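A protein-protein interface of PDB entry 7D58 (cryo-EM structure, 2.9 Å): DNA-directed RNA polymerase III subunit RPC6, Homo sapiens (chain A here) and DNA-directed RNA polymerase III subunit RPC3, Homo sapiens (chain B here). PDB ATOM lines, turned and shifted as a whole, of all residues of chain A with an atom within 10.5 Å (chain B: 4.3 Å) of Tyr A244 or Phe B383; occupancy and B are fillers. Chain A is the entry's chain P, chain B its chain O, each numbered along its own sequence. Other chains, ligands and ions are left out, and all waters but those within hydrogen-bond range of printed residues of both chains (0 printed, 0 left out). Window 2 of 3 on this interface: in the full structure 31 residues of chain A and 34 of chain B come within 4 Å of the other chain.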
ATOM      1  N   GLN A 170      17.811  35.675 -14.002  1.00  0.00           N
ATOM      2  CA  GLN A 170      18.404  34.343 -14.071  1.00  0.00           C
ATOM      3  C   GLN A 170      18.509  33.959 -15.544  1.00  0.00           C
ATOM      4  O   GLN A 170      17.502  33.659 -16.190  1.00  0.00           O
ATOM      5  CB  GLN A 170      17.576  33.330 -13.285  1.00  0.00           C
ATOM      6  CG  GLN A 170      18.132  31.916 -13.315  1.00  0.00           C
ATOM      7  CD  GLN A 170      19.498  31.811 -12.665  1.00  0.00           C
ATOM      8  OE1 GLN A 170      19.749  32.412 -11.620  1.00  0.00           O
ATOM      9  NE2 GLN A 170      20.390  31.044 -13.281  1.00  0.00           N
ATOM     10  N   VAL A 177      24.570  25.684 -21.501  1.00  0.00           N
ATOM     11  CA  VAL A 177      24.597  24.934 -20.243  1.00  0.00           C
ATOM     12  C   VAL A 177      25.058  23.501 -20.482  1.00  0.00           C
ATOM     13  O   VAL A 177      25.957  22.994 -19.802  1.00  0.00           O
ATOM     14  CB  VAL A 177      23.219  24.975 -19.559  1.00  0.00           C
ATOM     15  CG1 VAL A 177      23.143  23.936 -18.451  1.00  0.00           C
ATOM     16  CG2 VAL A 177      22.955  26.361 -18.995  1.00  0.00           C
ATOM     17  N   GLU A 178      24.453  22.827 -21.463  1.00  0.00           N
ATOM     18  CA  GLU A 178      24.805  21.433 -21.720  1.00  0.00           C
ATOM     19  C   GLU A 178      26.180  21.286 -22.369  1.00  0.00           C
ATOM     20  O   GLU A 178      26.850  20.267 -22.173  1.00  0.00           O
ATOM     21  CB  GLU A 178      23.720  20.742 -22.550  1.00  0.00           C
ATOM     22  CG  GLU A 178      22.679  19.964 -21.719  1.00  0.00           C
ATOM     23  CD  GLU A 178      21.603  20.815 -21.066  1.00  0.00           C
ATOM     24  OE1 GLU A 178      21.579  22.043 -21.275  1.00  0.00           O
ATOM     25  OE2 GLU A 178      20.774  20.241 -20.325  1.00  0.00           O
ATOM     26  N   ASN A 181      28.370  21.436 -19.519  1.00  0.00           N
ATOM     27  CA  ASN A 181      28.269  20.155 -18.828  1.00  0.00           C
ATOM     28  C   ASN A 181      29.131  19.097 -19.506  1.00  0.00           C
ATOM     29  O   ASN A 181      29.838  18.330 -18.841  1.00  0.00           O
ATOM     30  CB  ASN A 181      26.806  19.712 -18.778  1.00  0.00           C
ATOM     31  CG  ASN A 181      26.522  18.767 -17.629  1.00  0.00           C
ATOM     32  OD1 ASN A 181      27.273  18.707 -16.658  1.00  0.00           O
ATOM     33  ND2 ASN A 181      25.429  18.021 -17.734  1.00  0.00           N
ATOM     34  N   GLU A 233      28.168  28.451  -7.295  1.00  0.00           N
ATOM     35  CA  GLU A 233      26.863  27.828  -7.475  1.00  0.00           C
ATOM     36  C   GLU A 233      26.693  27.230  -8.863  1.00  0.00           C
ATOM     37  O   GLU A 233      26.103  26.155  -8.990  1.00  0.00           O
ATOM     38  CB  GLU A 233      25.728  28.819  -7.196  1.00  0.00           C
ATOM     39  CG  GLU A 233      25.673  30.022  -8.113  1.00  0.00           C
ATOM     40  CD  GLU A 233      26.301  31.235  -7.482  1.00  0.00           C
ATOM     41  OE1 GLU A 233      26.962  31.066  -6.437  1.00  0.00           O
ATOM     42  OE2 GLU A 233      26.127  32.350  -8.018  1.00  0.00           O
ATOM     43  N   ASP A 234      27.204  27.883  -9.910  1.00  0.00           N
ATOM     44  CA  ASP A 234      27.023  27.338 -11.254  1.00  0.00           C
ATOM     45  C   ASP A 234      27.712  25.986 -11.399  1.00  0.00           C
ATOM     46  O   ASP A 234      27.109  25.028 -11.895  1.00  0.00           O
ATOM     47  CB  ASP A 234      27.531  28.321 -12.311  1.00  0.00           C
ATOM     48  CG  ASP A 234      26.773  29.636 -12.303  1.00  0.00           C
ATOM     49  OD1 ASP A 234      25.574  29.635 -11.954  1.00  0.00           O
ATOM     50  OD2 ASP A 234      27.376  30.670 -12.666  1.00  0.00           O
ATOM     51  N   ILE A 235      28.962  25.875 -10.938  1.00  0.00           N
ATOM     52  CA  ILE A 235      29.684  24.613 -11.089  1.00  0.00           C
ATOM     53  C   ILE A 235      29.085  23.540 -10.185  1.00  0.00           C
ATOM     54  O   ILE A 235      28.978  22.370 -10.577  1.00  0.00           O
ATOM     55  CB  ILE A 235      31.193  24.803 -10.836  1.00  0.00           C
ATOM     56  CG1 ILE A 235      31.481  25.316  -9.424  1.00  0.00           C
ATOM     57  CG2 ILE A 235      31.796  25.731 -11.875  1.00  0.00           C
ATOM     58  CD1 ILE A 235      32.955  25.469  -9.137  1.00  0.00           C
ATOM     59  N   GLU A 236      28.656  23.916  -8.974  1.00  0.00           N
ATOM     60  CA  GLU A 236      28.115  22.897  -8.080  1.00  0.00           C
ATOM     61  C   GLU A 236      26.754  22.414  -8.573  1.00  0.00           C
ATOM     62  O   GLU A 236      26.433  21.226  -8.464  1.00  0.00           O
ATOM     63  CB  GLU A 236      28.046  23.421  -6.644  1.00  0.00           C
ATOM     64  CG  GLU A 236      27.011  24.487  -6.377  1.00  0.00           C
ATOM     65  CD  GLU A 236      25.710  23.907  -5.870  1.00  0.00           C
ATOM     66  OE1 GLU A 236      25.729  22.769  -5.357  1.00  0.00           O
ATOM     67  OE2 GLU A 236      24.669  24.585  -5.978  1.00  0.00           O
ATOM     68  N   THR A 237      25.961  23.307  -9.179  1.00  0.00           N
ATOM     69  CA  THR A 237      24.696  22.886  -9.775  1.00  0.00           C
ATOM     70  C   THR A 237      24.914  22.060 -11.035  1.00  0.00           C
ATOM     71  O   THR A 237      24.153  21.128 -11.302  1.00  0.00           O
ATOM     72  CB  THR A 237      23.814  24.098 -10.090  1.00  0.00           C
ATOM     73  OG1 THR A 237      24.556  25.052 -10.861  1.00  0.00           O
ATOM     74  CG2 THR A 237      23.281  24.741  -8.821  1.00  0.00           C
ATOM     75  N   ILE A 238      25.924  22.393 -11.841  1.00  0.00           N
ATOM     76  CA  ILE A 238      26.192  21.582 -13.023  1.00  0.00           C
ATOM     77  C   ILE A 238      26.640  20.184 -12.613  1.00  0.00           C
ATOM     78  O   ILE A 238      26.230  19.181 -13.212  1.00  0.00           O
ATOM     79  CB  ILE A 238      27.226  22.277 -13.928  1.00  0.00           C
ATOM     80  CG1 ILE A 238      26.592  23.474 -14.644  1.00  0.00           C
ATOM     81  CG2 ILE A 238      27.791  21.299 -14.938  1.00  0.00           C
ATOM     82  CD1 ILE A 238      25.477  23.103 -15.603  1.00  0.00           C
ATOM     83  N   LEU A 239      27.464  20.088 -11.568  1.00  0.00           N
ATOM     84  CA  LEU A 239      27.849  18.778 -11.059  1.00  0.00           C
ATOM     85  C   LEU A 239      26.659  18.065 -10.424  1.00  0.00           C
ATOM     86  O   LEU A 239      26.587  16.831 -10.432  1.00  0.00           O
ATOM     87  CB  LEU A 239      29.009  18.928 -10.075  1.00  0.00           C
ATOM     88  CG  LEU A 239      30.321  19.321 -10.763  1.00  0.00           C
ATOM     89  CD1 LEU A 239      31.330  19.885  -9.780  1.00  0.00           C
ATOM     90  CD2 LEU A 239      30.912  18.132 -11.507  1.00  0.00           C
ATOM     91  N   ASN A 240      25.695  18.825  -9.895  1.00  0.00           N
ATOM     92  CA  ASN A 240      24.445  18.218  -9.447  1.00  0.00           C
ATOM     93  C   ASN A 240      23.648  17.637 -10.613  1.00  0.00           C
ATOM     94  O   ASN A 240      23.149  16.512 -10.518  1.00  0.00           O
ATOM     95  CB  ASN A 240      23.600  19.243  -8.688  1.00  0.00           C
ATOM     96  CG  ASN A 240      24.124  19.515  -7.289  1.00  0.00           C
ATOM     97  OD1 ASN A 240      24.697  18.635  -6.646  1.00  0.00           O
ATOM     98  ND2 ASN A 240      23.925  20.738  -6.809  1.00  0.00           N
ATOM     99  N   THR A 241      23.513  18.384 -11.710  1.00  0.00           N
ATOM    100  CA  THR A 241      22.837  17.852 -12.894  1.00  0.00           C
ATOM    101  C   THR A 241      23.576  16.643 -13.448  1.00  0.00           C
ATOM    102  O   THR A 241      22.969  15.770 -14.079  1.00  0.00           O
ATOM    103  CB  THR A 241      22.698  18.926 -13.977  1.00  0.00           C
ATOM    104  OG1 THR A 241      23.966  19.144 -14.609  1.00  0.00           O
ATOM    105  CG2 THR A 241      22.170  20.230 -13.402  1.00  0.00           C
ATOM    106  N   LEU A 242      24.891  16.584 -13.233  1.00  0.00           N
ATOM    107  CA  LEU A 242      25.672  15.418 -13.624  1.00  0.00           C
ATOM    108  C   LEU A 242      25.421  14.209 -12.733  1.00  0.00           C
ATOM    109  O   LEU A 242      25.308  13.091 -13.251  1.00  0.00           O
ATOM    110  CB  LEU A 242      27.165  15.753 -13.611  1.00  0.00           C
ATOM    111  CG  LEU A 242      27.819  16.059 -14.958  1.00  0.00           C
ATOM    112  CD1 LEU A 242      29.326  16.195 -14.799  1.00  0.00           C
ATOM    113  CD2 LEU A 242      27.479  14.981 -15.975  1.00  0.00           C
ATOM    114  N   ILE A 243      25.345  14.396 -11.414  1.00  0.00           N
ATOM    115  CA  ILE A 243      25.055  13.263 -10.537  1.00  0.00           C
ATOM    116  C   ILE A 243      23.614  12.806 -10.726  1.00  0.00           C
ATOM    117  O   ILE A 243      23.278  11.642 -10.469  1.00  0.00           O
ATOM    118  CB  ILE A 243      25.358  13.603  -9.063  1.00  0.00           C
ATOM    119  CG1 ILE A 243      24.336  14.592  -8.499  1.00  0.00           C
ATOM    120  CG2 ILE A 243      26.775  14.134  -8.908  1.00  0.00           C
ATOM    121  CD1 ILE A 243      24.489  14.850  -7.017  1.00  0.00           C
ATOM    122  N   TYR A 244      22.738  13.707 -11.179  1.00  0.00           N
ATOM    123  CA  TYR A 244      21.392  13.293 -11.563  1.00  0.00           C
ATOM    124  C   TYR A 244      21.416  12.433 -12.819  1.00  0.00           C
ATOM    125  O   TYR A 244      20.581  11.535 -12.969  1.00  0.00           O
ATOM    126  CB  TYR A 244      20.496  14.514 -11.778  1.00  0.00           C
ATOM    127  CG  TYR A 244      20.382  15.423 -10.575  1.00  0.00           C
ATOM    128  CD1 TYR A 244      20.457  14.914  -9.285  1.00  0.00           C
ATOM    129  CD2 TYR A 244      20.207  16.792 -10.729  1.00  0.00           C
ATOM    130  CE1 TYR A 244      20.358  15.742  -8.183  1.00  0.00           C
ATOM    131  CE2 TYR A 244      20.112  17.629  -9.633  1.00  0.00           C
ATOM    132  CZ  TYR A 244      20.185  17.099  -8.363  1.00  0.00           C
ATOM    133  OH  TYR A 244      20.085  17.926  -7.268  1.00  0.00           O
ATOM    134  N   ASP A 245      22.359  12.695 -13.728  1.00  0.00           N
ATOM    135  CA  ASP A 245      22.499  11.857 -14.914  1.00  0.00           C
ATOM    136  C   ASP A 245      22.996  10.465 -14.546  1.00  0.00           C
ATOM    137  O   ASP A 245      22.657   9.479 -15.211  1.00  0.00           O
ATOM    138  CB  ASP A 245      23.454  12.513 -15.912  1.00  0.00           C
ATOM    139  CG  ASP A 245      22.810  13.652 -16.676  1.00  0.00           C
ATOM    140  OD1 ASP A 245      23.543  14.410 -17.345  1.00  0.00           O
ATOM    141  OD2 ASP A 245      21.572  13.790 -16.609  1.00  0.00           O
ATOM    142  N   GLY A 246      23.806  10.365 -13.493  1.00  0.00           N
ATOM    143  CA  GLY A 246      24.384   9.099 -13.093  1.00  0.00           C
ATOM    144  C   GLY A 246      25.738   8.862 -13.728  1.00  0.00           C
ATOM    145  O   GLY A 246      26.040   7.751 -14.176  1.00  0.00           O
ATOM    146  N   LYS A 247      26.564   9.905 -13.770  1.00  0.00           N
ATOM    147  CA  LYS A 247      27.875   9.825 -14.408  1.00  0.00           C
ATOM    148  C   LYS A 247      29.039  10.129 -13.476  1.00  0.00           C
ATOM    149  O   LYS A 247      30.122   9.569 -13.678  1.00  0.00           O
ATOM    150  CB  LYS A 247      27.937  10.779 -15.609  1.00  0.00           C
ATOM    151  CG  LYS A 247      26.912  10.475 -16.690  1.00  0.00           C
ATOM    152  CD  LYS A 247      26.768  11.632 -17.668  1.00  0.00           C
ATOM    153  CE  LYS A 247      27.912  11.666 -18.668  1.00  0.00           C
ATOM    154  NZ  LYS A 247      27.866  10.510 -19.607  1.00  0.00           N
ATOM    155  N   VAL A 248      28.873  10.990 -12.476  1.00  0.00           N
ATOM    156  CA  VAL A 248      29.911  11.297 -11.499  1.00  0.00           C
ATOM    157  C   VAL A 248      29.266  11.305 -10.121  1.00  0.00           C
ATOM    158  O   VAL A 248      28.040  11.415 -10.009  1.00  0.00           O
ATOM    159  CB  VAL A 248      30.591  12.648 -11.793  1.00  0.00           C
ATOM    160  CG1 VAL A 248      31.277  12.620 -13.152  1.00  0.00           C
ATOM    161  CG2 VAL A 248      29.574  13.774 -11.730  1.00  0.00           C
ATOM    162  N   GLU A 249      30.084  11.175  -9.079  1.00  0.00           N
ATOM    163  CA  GLU A 249      29.610  11.235  -7.702  1.00  0.00           C
ATOM    164  C   GLU A 249      30.383  12.302  -6.940  1.00  0.00           C
ATOM    165  O   GLU A 249      31.542  12.587  -7.261  1.00  0.00           O
ATOM    166  CB  GLU A 249      29.741   9.874  -7.008  1.00  0.00           C
ATOM    167  CG  GLU A 249      31.163   9.364  -6.811  1.00  0.00           C
ATOM    168  CD  GLU A 249      31.745   9.747  -5.461  1.00  0.00           C
ATOM    169  OE1 GLU A 249      30.960  10.075  -4.548  1.00  0.00           O
ATOM    170  OE2 GLU A 249      32.985   9.708  -5.310  1.00  0.00           O
ATOM    171  N   MET A 250      29.733  12.910  -5.954  1.00  0.00           N
ATOM    172  CA  MET A 250      30.366  13.907  -5.103  1.00  0.00           C
ATOM    173  C   MET A 250      30.477  13.359  -3.688  1.00  0.00           C
ATOM    174  O   MET A 250      29.713  12.467  -3.303  1.00  0.00           O
ATOM    175  CB  MET A 250      29.574  15.219  -5.108  1.00  0.00           C
ATOM    176  CG  MET A 250      28.178  15.160  -4.488  1.00  0.00           C
ATOM    177  SD  MET A 250      28.117  15.469  -2.706  1.00  0.00           S
ATOM    178  CE  MET A 250      28.403  17.240  -2.662  1.00  0.00           C
ATOM    179  N   TYR A 270      34.966  15.475  -6.253  1.00  0.00           N
ATOM    180  CA  TYR A 270      34.161  14.844  -7.285  1.00  0.00           C
ATOM    181  C   TYR A 270      34.958  13.742  -7.968  1.00  0.00           C
ATOM    182  O   TYR A 270      36.103  13.943  -8.382  1.00  0.00           O
ATOM    183  CB  TYR A 270      33.686  15.875  -8.316  1.00  0.00           C
ATOM    184  CG  TYR A 270      32.801  16.936  -7.709  1.00  0.00           C
ATOM    185  CD1 TYR A 270      31.422  16.786  -7.691  1.00  0.00           C
ATOM    186  CD2 TYR A 270      33.343  18.082  -7.142  1.00  0.00           C
ATOM    187  CE1 TYR A 270      30.606  17.748  -7.130  1.00  0.00           C
ATOM    188  CE2 TYR A 270      32.536  19.050  -6.576  1.00  0.00           C
ATOM    189  CZ  TYR A 270      31.168  18.878  -6.573  1.00  0.00           C
ATOM    190  OH  TYR A 270      30.357  19.838  -6.015  1.00  0.00           O
ATOM    191  N   VAL A 273      32.457   8.053 -11.972  1.00  0.00           N
ATOM    192  CA  VAL A 273      31.994   6.677 -11.834  1.00  0.00           C
ATOM    193  C   VAL A 273      31.471   6.186 -13.178  1.00  0.00           C
ATOM    194  O   VAL A 273      30.991   6.977 -13.998  1.00  0.00           O
ATOM    195  CB  VAL A 273      30.911   6.567 -10.747  1.00  0.00           C
ATOM    196  CG1 VAL A 273      31.511   6.838  -9.379  1.00  0.00           C
ATOM    197  CG2 VAL A 273      29.766   7.527 -11.035  1.00  0.00           C
ATOM    198  N   ARG B 364      17.257  11.600 -16.113  1.00  0.00           N
ATOM    199  CA  ARG B 364      17.865  12.513 -15.151  1.00  0.00           C
ATOM    200  C   ARG B 364      16.851  12.983 -14.118  1.00  0.00           C
ATOM    201  O   ARG B 364      17.133  12.941 -12.915  1.00  0.00           O
ATOM    202  CB  ARG B 364      18.479  13.712 -15.876  1.00  0.00           C
ATOM    203  CG  ARG B 364      18.572  14.978 -15.034  1.00  0.00           C
ATOM    204  CD  ARG B 364      18.848  16.201 -15.896  1.00  0.00           C
ATOM    205  NE  ARG B 364      20.071  16.055 -16.681  1.00  0.00           N
ATOM    206  CZ  ARG B 364      20.406  16.845 -17.696  1.00  0.00           C
ATOM    207  NH1 ARG B 364      19.609  17.842 -18.056  1.00  0.00           N
ATOM    208  NH2 ARG B 364      21.540  16.638 -18.354  1.00  0.00           N
ATOM    209  N   ARG B 367      15.929  10.012 -11.791  1.00  0.00           N
ATOM    210  CA  ARG B 367      16.899   9.837 -10.715  1.00  0.00           C
ATOM    211  C   ARG B 367      16.855  10.984  -9.713  1.00  0.00           C
ATOM    212  O   ARG B 367      17.044  10.759  -8.512  1.00  0.00           O
ATOM    213  CB  ARG B 367      18.304   9.685 -11.300  1.00  0.00           C
ATOM    214  CG  ARG B 367      18.430   8.478 -12.212  1.00  0.00           C
ATOM    215  CD  ARG B 367      19.772   8.396 -12.919  1.00  0.00           C
ATOM    216  NE  ARG B 367      19.686   7.568 -14.120  1.00  0.00           N
ATOM    217  CZ  ARG B 367      20.736   7.080 -14.774  1.00  0.00           C
ATOM    218  NH1 ARG B 367      21.962   7.332 -14.341  1.00  0.00           N
ATOM    219  NH2 ARG B 367      20.561   6.338 -15.859  1.00  0.00           N
ATOM    220  N   LEU B 368      16.596  12.209 -10.179  1.00  0.00           N
ATOM    221  CA  LEU B 368      16.483  13.343  -9.268  1.00  0.00           C
ATOM    222  C   LEU B 368      15.332  13.162  -8.288  1.00  0.00           C
ATOM    223  O   LEU B 368      15.487  13.442  -7.094  1.00  0.00           O
ATOM    224  CB  LEU B 368      16.293  14.635 -10.065  1.00  0.00           C
ATOM    225  CG  LEU B 368      16.311  15.990  -9.344  1.00  0.00           C
ATOM    226  CD1 LEU B 368      16.790  17.072 -10.293  1.00  0.00           C
ATOM    227  CD2 LEU B 368      14.943  16.362  -8.785  1.00  0.00           C
ATOM    228  N   LYS B 372      15.572  12.626  -4.129  1.00  0.00           N
ATOM    229  CA  LYS B 372      14.759  13.476  -3.260  1.00  0.00           C
ATOM    230  C   LYS B 372      13.326  12.961  -3.293  1.00  0.00           C
ATOM    231  O   LYS B 372      12.545  13.277  -4.192  1.00  0.00           O
ATOM    232  CB  LYS B 372      14.840  14.932  -3.698  1.00  0.00           C
ATOM    233  CG  LYS B 372      16.253  15.482  -3.777  1.00  0.00           C
ATOM    234  CD  LYS B 372      16.307  16.721  -4.654  1.00  0.00           C
ATOM    235  CE  LYS B 372      17.714  16.974  -5.170  1.00  0.00           C
ATOM    236  NZ  LYS B 372      17.705  17.697  -6.470  1.00  0.00           N
ATOM    237  N   ILE B 375       9.022  15.128  -3.858  1.00  0.00           N
ATOM    238  CA  ILE B 375       9.314  16.490  -4.281  1.00  0.00           C
ATOM    239  C   ILE B 375       8.071  17.086  -4.932  1.00  0.00           C
ATOM    240  O   ILE B 375       7.189  16.375  -5.419  1.00  0.00           O
ATOM    241  CB  ILE B 375      10.530  16.540  -5.231  1.00  0.00           C
ATOM    242  CG1 ILE B 375      11.255  17.880  -5.095  1.00  0.00           C
ATOM    243  CG2 ILE B 375      10.102  16.298  -6.672  1.00  0.00           C
ATOM    244  CD1 ILE B 375      12.548  17.960  -5.875  1.00  0.00           C
ATOM    245  N   GLN B 379       9.246  23.043  -7.412  1.00  0.00           N
ATOM    246  CA  GLN B 379      10.592  22.960  -6.855  1.00  0.00           C
ATOM    247  C   GLN B 379      11.473  21.936  -7.552  1.00  0.00           C
ATOM    248  O   GLN B 379      12.658  21.837  -7.219  1.00  0.00           O
ATOM    249  CB  GLN B 379      10.544  22.628  -5.361  1.00  0.00           C
ATOM    250  CG  GLN B 379       9.598  23.489  -4.552  1.00  0.00           C
ATOM    251  CD  GLN B 379      10.012  24.947  -4.526  1.00  0.00           C
ATOM    252  OE1 GLN B 379      11.195  25.264  -4.401  1.00  0.00           O
ATOM    253  NE2 GLN B 379       9.038  25.842  -4.643  1.00  0.00           N
ATOM    254  N   VAL B 380      10.934  21.148  -8.481  1.00  0.00           N
ATOM    255  CA  VAL B 380      11.795  20.220  -9.205  1.00  0.00           C
ATOM    256  C   VAL B 380      12.596  20.954 -10.280  1.00  0.00           C
ATOM    257  O   VAL B 380      13.694  20.518 -10.648  1.00  0.00           O
ATOM    258  CB  VAL B 380      10.969  19.056  -9.787  1.00  0.00           C
ATOM    259  CG1 VAL B 380      10.078  19.523 -10.930  1.00  0.00           C
ATOM    260  CG2 VAL B 380      11.875  17.918 -10.232  1.00  0.00           C
ATOM    261  N   GLU B 381      12.085  22.083 -10.781  1.00  0.00           N
ATOM    262  CA  GLU B 381      12.747  22.771 -11.886  1.00  0.00           C
ATOM    263  C   GLU B 381      13.899  23.654 -11.416  1.00  0.00           C
ATOM    264  O   GLU B 381      14.842  23.897 -12.180  1.00  0.00           O
ATOM    265  CB  GLU B 381      11.734  23.607 -12.663  1.00  0.00           C
ATOM    266  CG  GLU B 381      12.284  24.118 -13.980  1.00  0.00           C
ATOM    267  CD  GLU B 381      11.295  24.961 -14.750  1.00  0.00           C
ATOM    268  OE1 GLU B 381      10.222  25.279 -14.194  1.00  0.00           O
ATOM    269  OE2 GLU B 381      11.596  25.301 -15.916  1.00  0.00           O
ATOM    270  N   ASP B 382      13.839  24.164 -10.184  1.00  0.00           N
ATOM    271  CA  ASP B 382      14.960  24.942  -9.666  1.00  0.00           C
ATOM    272  C   ASP B 382      16.187  24.059  -9.456  1.00  0.00           C
ATOM    273  O   ASP B 382      17.324  24.541  -9.483  1.00  0.00           O
ATOM    274  CB  ASP B 382      14.552  25.664  -8.375  1.00  0.00           C
ATOM    275  CG  ASP B 382      14.114  24.717  -7.265  1.00  0.00           C
ATOM    276  OD1 ASP B 382      14.641  23.589  -7.173  1.00  0.00           O
ATOM    277  OD2 ASP B 382      13.219  25.099  -6.481  1.00  0.00           O
ATOM    278  N   PHE B 383      15.965  22.762  -9.227  1.00  0.00           N
ATOM    279  CA  PHE B 383      17.062  21.802  -9.198  1.00  0.00           C
ATOM    280  C   PHE B 383      17.488  21.427 -10.614  1.00  0.00           C
ATOM    281  O   PHE B 383      18.618  21.701 -11.034  1.00  0.00           O
ATOM    282  CB  PHE B 383      16.635  20.557  -8.417  1.00  0.00           C
ATOM    283  CG  PHE B 383      16.775  20.694  -6.927  1.00  0.00           C
ATOM    284  CD1 PHE B 383      17.999  21.003  -6.355  1.00  0.00           C
ATOM    285  CD2 PHE B 383      15.678  20.520  -6.097  1.00  0.00           C
ATOM    286  CE1 PHE B 383      18.130  21.130  -4.980  1.00  0.00           C
ATOM    287  CE2 PHE B 383      15.802  20.645  -4.723  1.00  0.00           C
ATOM    288  CZ  PHE B 383      17.028  20.951  -4.164  1.00  0.00           C
ATOM    289  N   ALA B 384      16.583  20.813 -11.372  1.00  0.00           N
ATOM    290  CA  ALA B 384      16.884  20.352 -12.723  1.00  0.00           C
ATOM    291  C   ALA B 384      16.770  21.520 -13.693  1.00  0.00           C
ATOM    292  O   ALA B 384      15.670  22.023 -13.943  1.00  0.00           O
ATOM    293  CB  ALA B 384      15.944  19.220 -13.121  1.00  0.00           C
ATOM    294  N   MET B 385      17.899  21.934 -14.266  1.00  0.00           N
ATOM    295  CA  MET B 385      17.907  23.035 -15.221  1.00  0.00           C
ATOM    296  C   MET B 385      17.316  22.593 -16.555  1.00  0.00           C
ATOM    297  O   MET B 385      18.050  22.297 -17.503  1.00  0.00           O
ATOM    298  CB  MET B 385      19.332  23.557 -15.414  1.00  0.00           C
ATOM    299  CG  MET B 385      20.005  24.042 -14.133  1.00  0.00           C
ATOM    300  SD  MET B 385      19.192  25.473 -13.394  1.00  0.00           S
ATOM    301  CE  MET B 385      19.235  26.629 -14.761  1.00  0.00           C
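The guanidinium group (NH1) of Arg B364 lies within salt-bridge range of the side-chain carboxylate (OE2) of Glu A178 (3.5 Å).
NE of Arg B364 is in salt-bridge range of OD2 of Asp A245, at 2.7 Å.
The backbone carbonyl oxygen (O) of Asp A245 is in hydrogen-bond range of the guanidinium group (NH1) of Arg B367.
OH of Tyr A244 lies within hydrogen-bond range of NZ of Lys B372 (2.5 Å).
The backbone carbonyl oxygen (O) of Ile A238 lies within hydrogen-bond range of the side-chain hydroxyl (OG1) of Thr A241 (2.7 Å).
Among the printed residues, pairs that only touch across the chains: Tyr A244 with Arg B367 (3.2 Å), Gly A246 with Arg B367 (3.2 Å), Tyr A244 with Leu B368 (3.4 Å), Tyr A244 with Arg B364 (3.6 Å), Tyr A244 with Phe B383 (3.8 Å) and Thr A241 with Arg B364 (3.9 Å).
Of the printed residues of chain B, Thr A241 touches Arg B364 (3.9 Å).
Of the printed residues of chain B, Gly A246 touches Arg B367 (3.2 Å).
Arg B367 touches just these residues of chain A: Tyr A244 (3.2 Å), Asp A245 (2.4 Å) and Gly A246 (3.2 Å).
Leu B368 touches just one residue of chain A: Tyr A244 (3.4 Å).
Val B380 touches none of the printed residues of chain A.
Of chain A, only Tyr A244 comes within 4 Å of Phe B383.
No residue of chain A comes within 4 Å of Ala B384.
The nearest printed residue of chain B that does not touch Tyr A244 is Ala B384 (5.1 Å).
The nearest residue of chain A that does not touch Phe B383 is Thr A241 (4.5 Å).
The nearest printed residue of chain B that does not touch Gly A246 is Arg B364 (6.5 Å).
Of the 24 printed residues of chain A, 5 touch a printed residue of chain B.
Of the 12 printed residues of chain B, 5 touch a printed residue of chain A.
Hydrophobic or aromatic side chains of chain B that line the printed part of chain A: Leu B368 and Phe B383.
Among the printed residues, 10 pairs touch across the chains.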
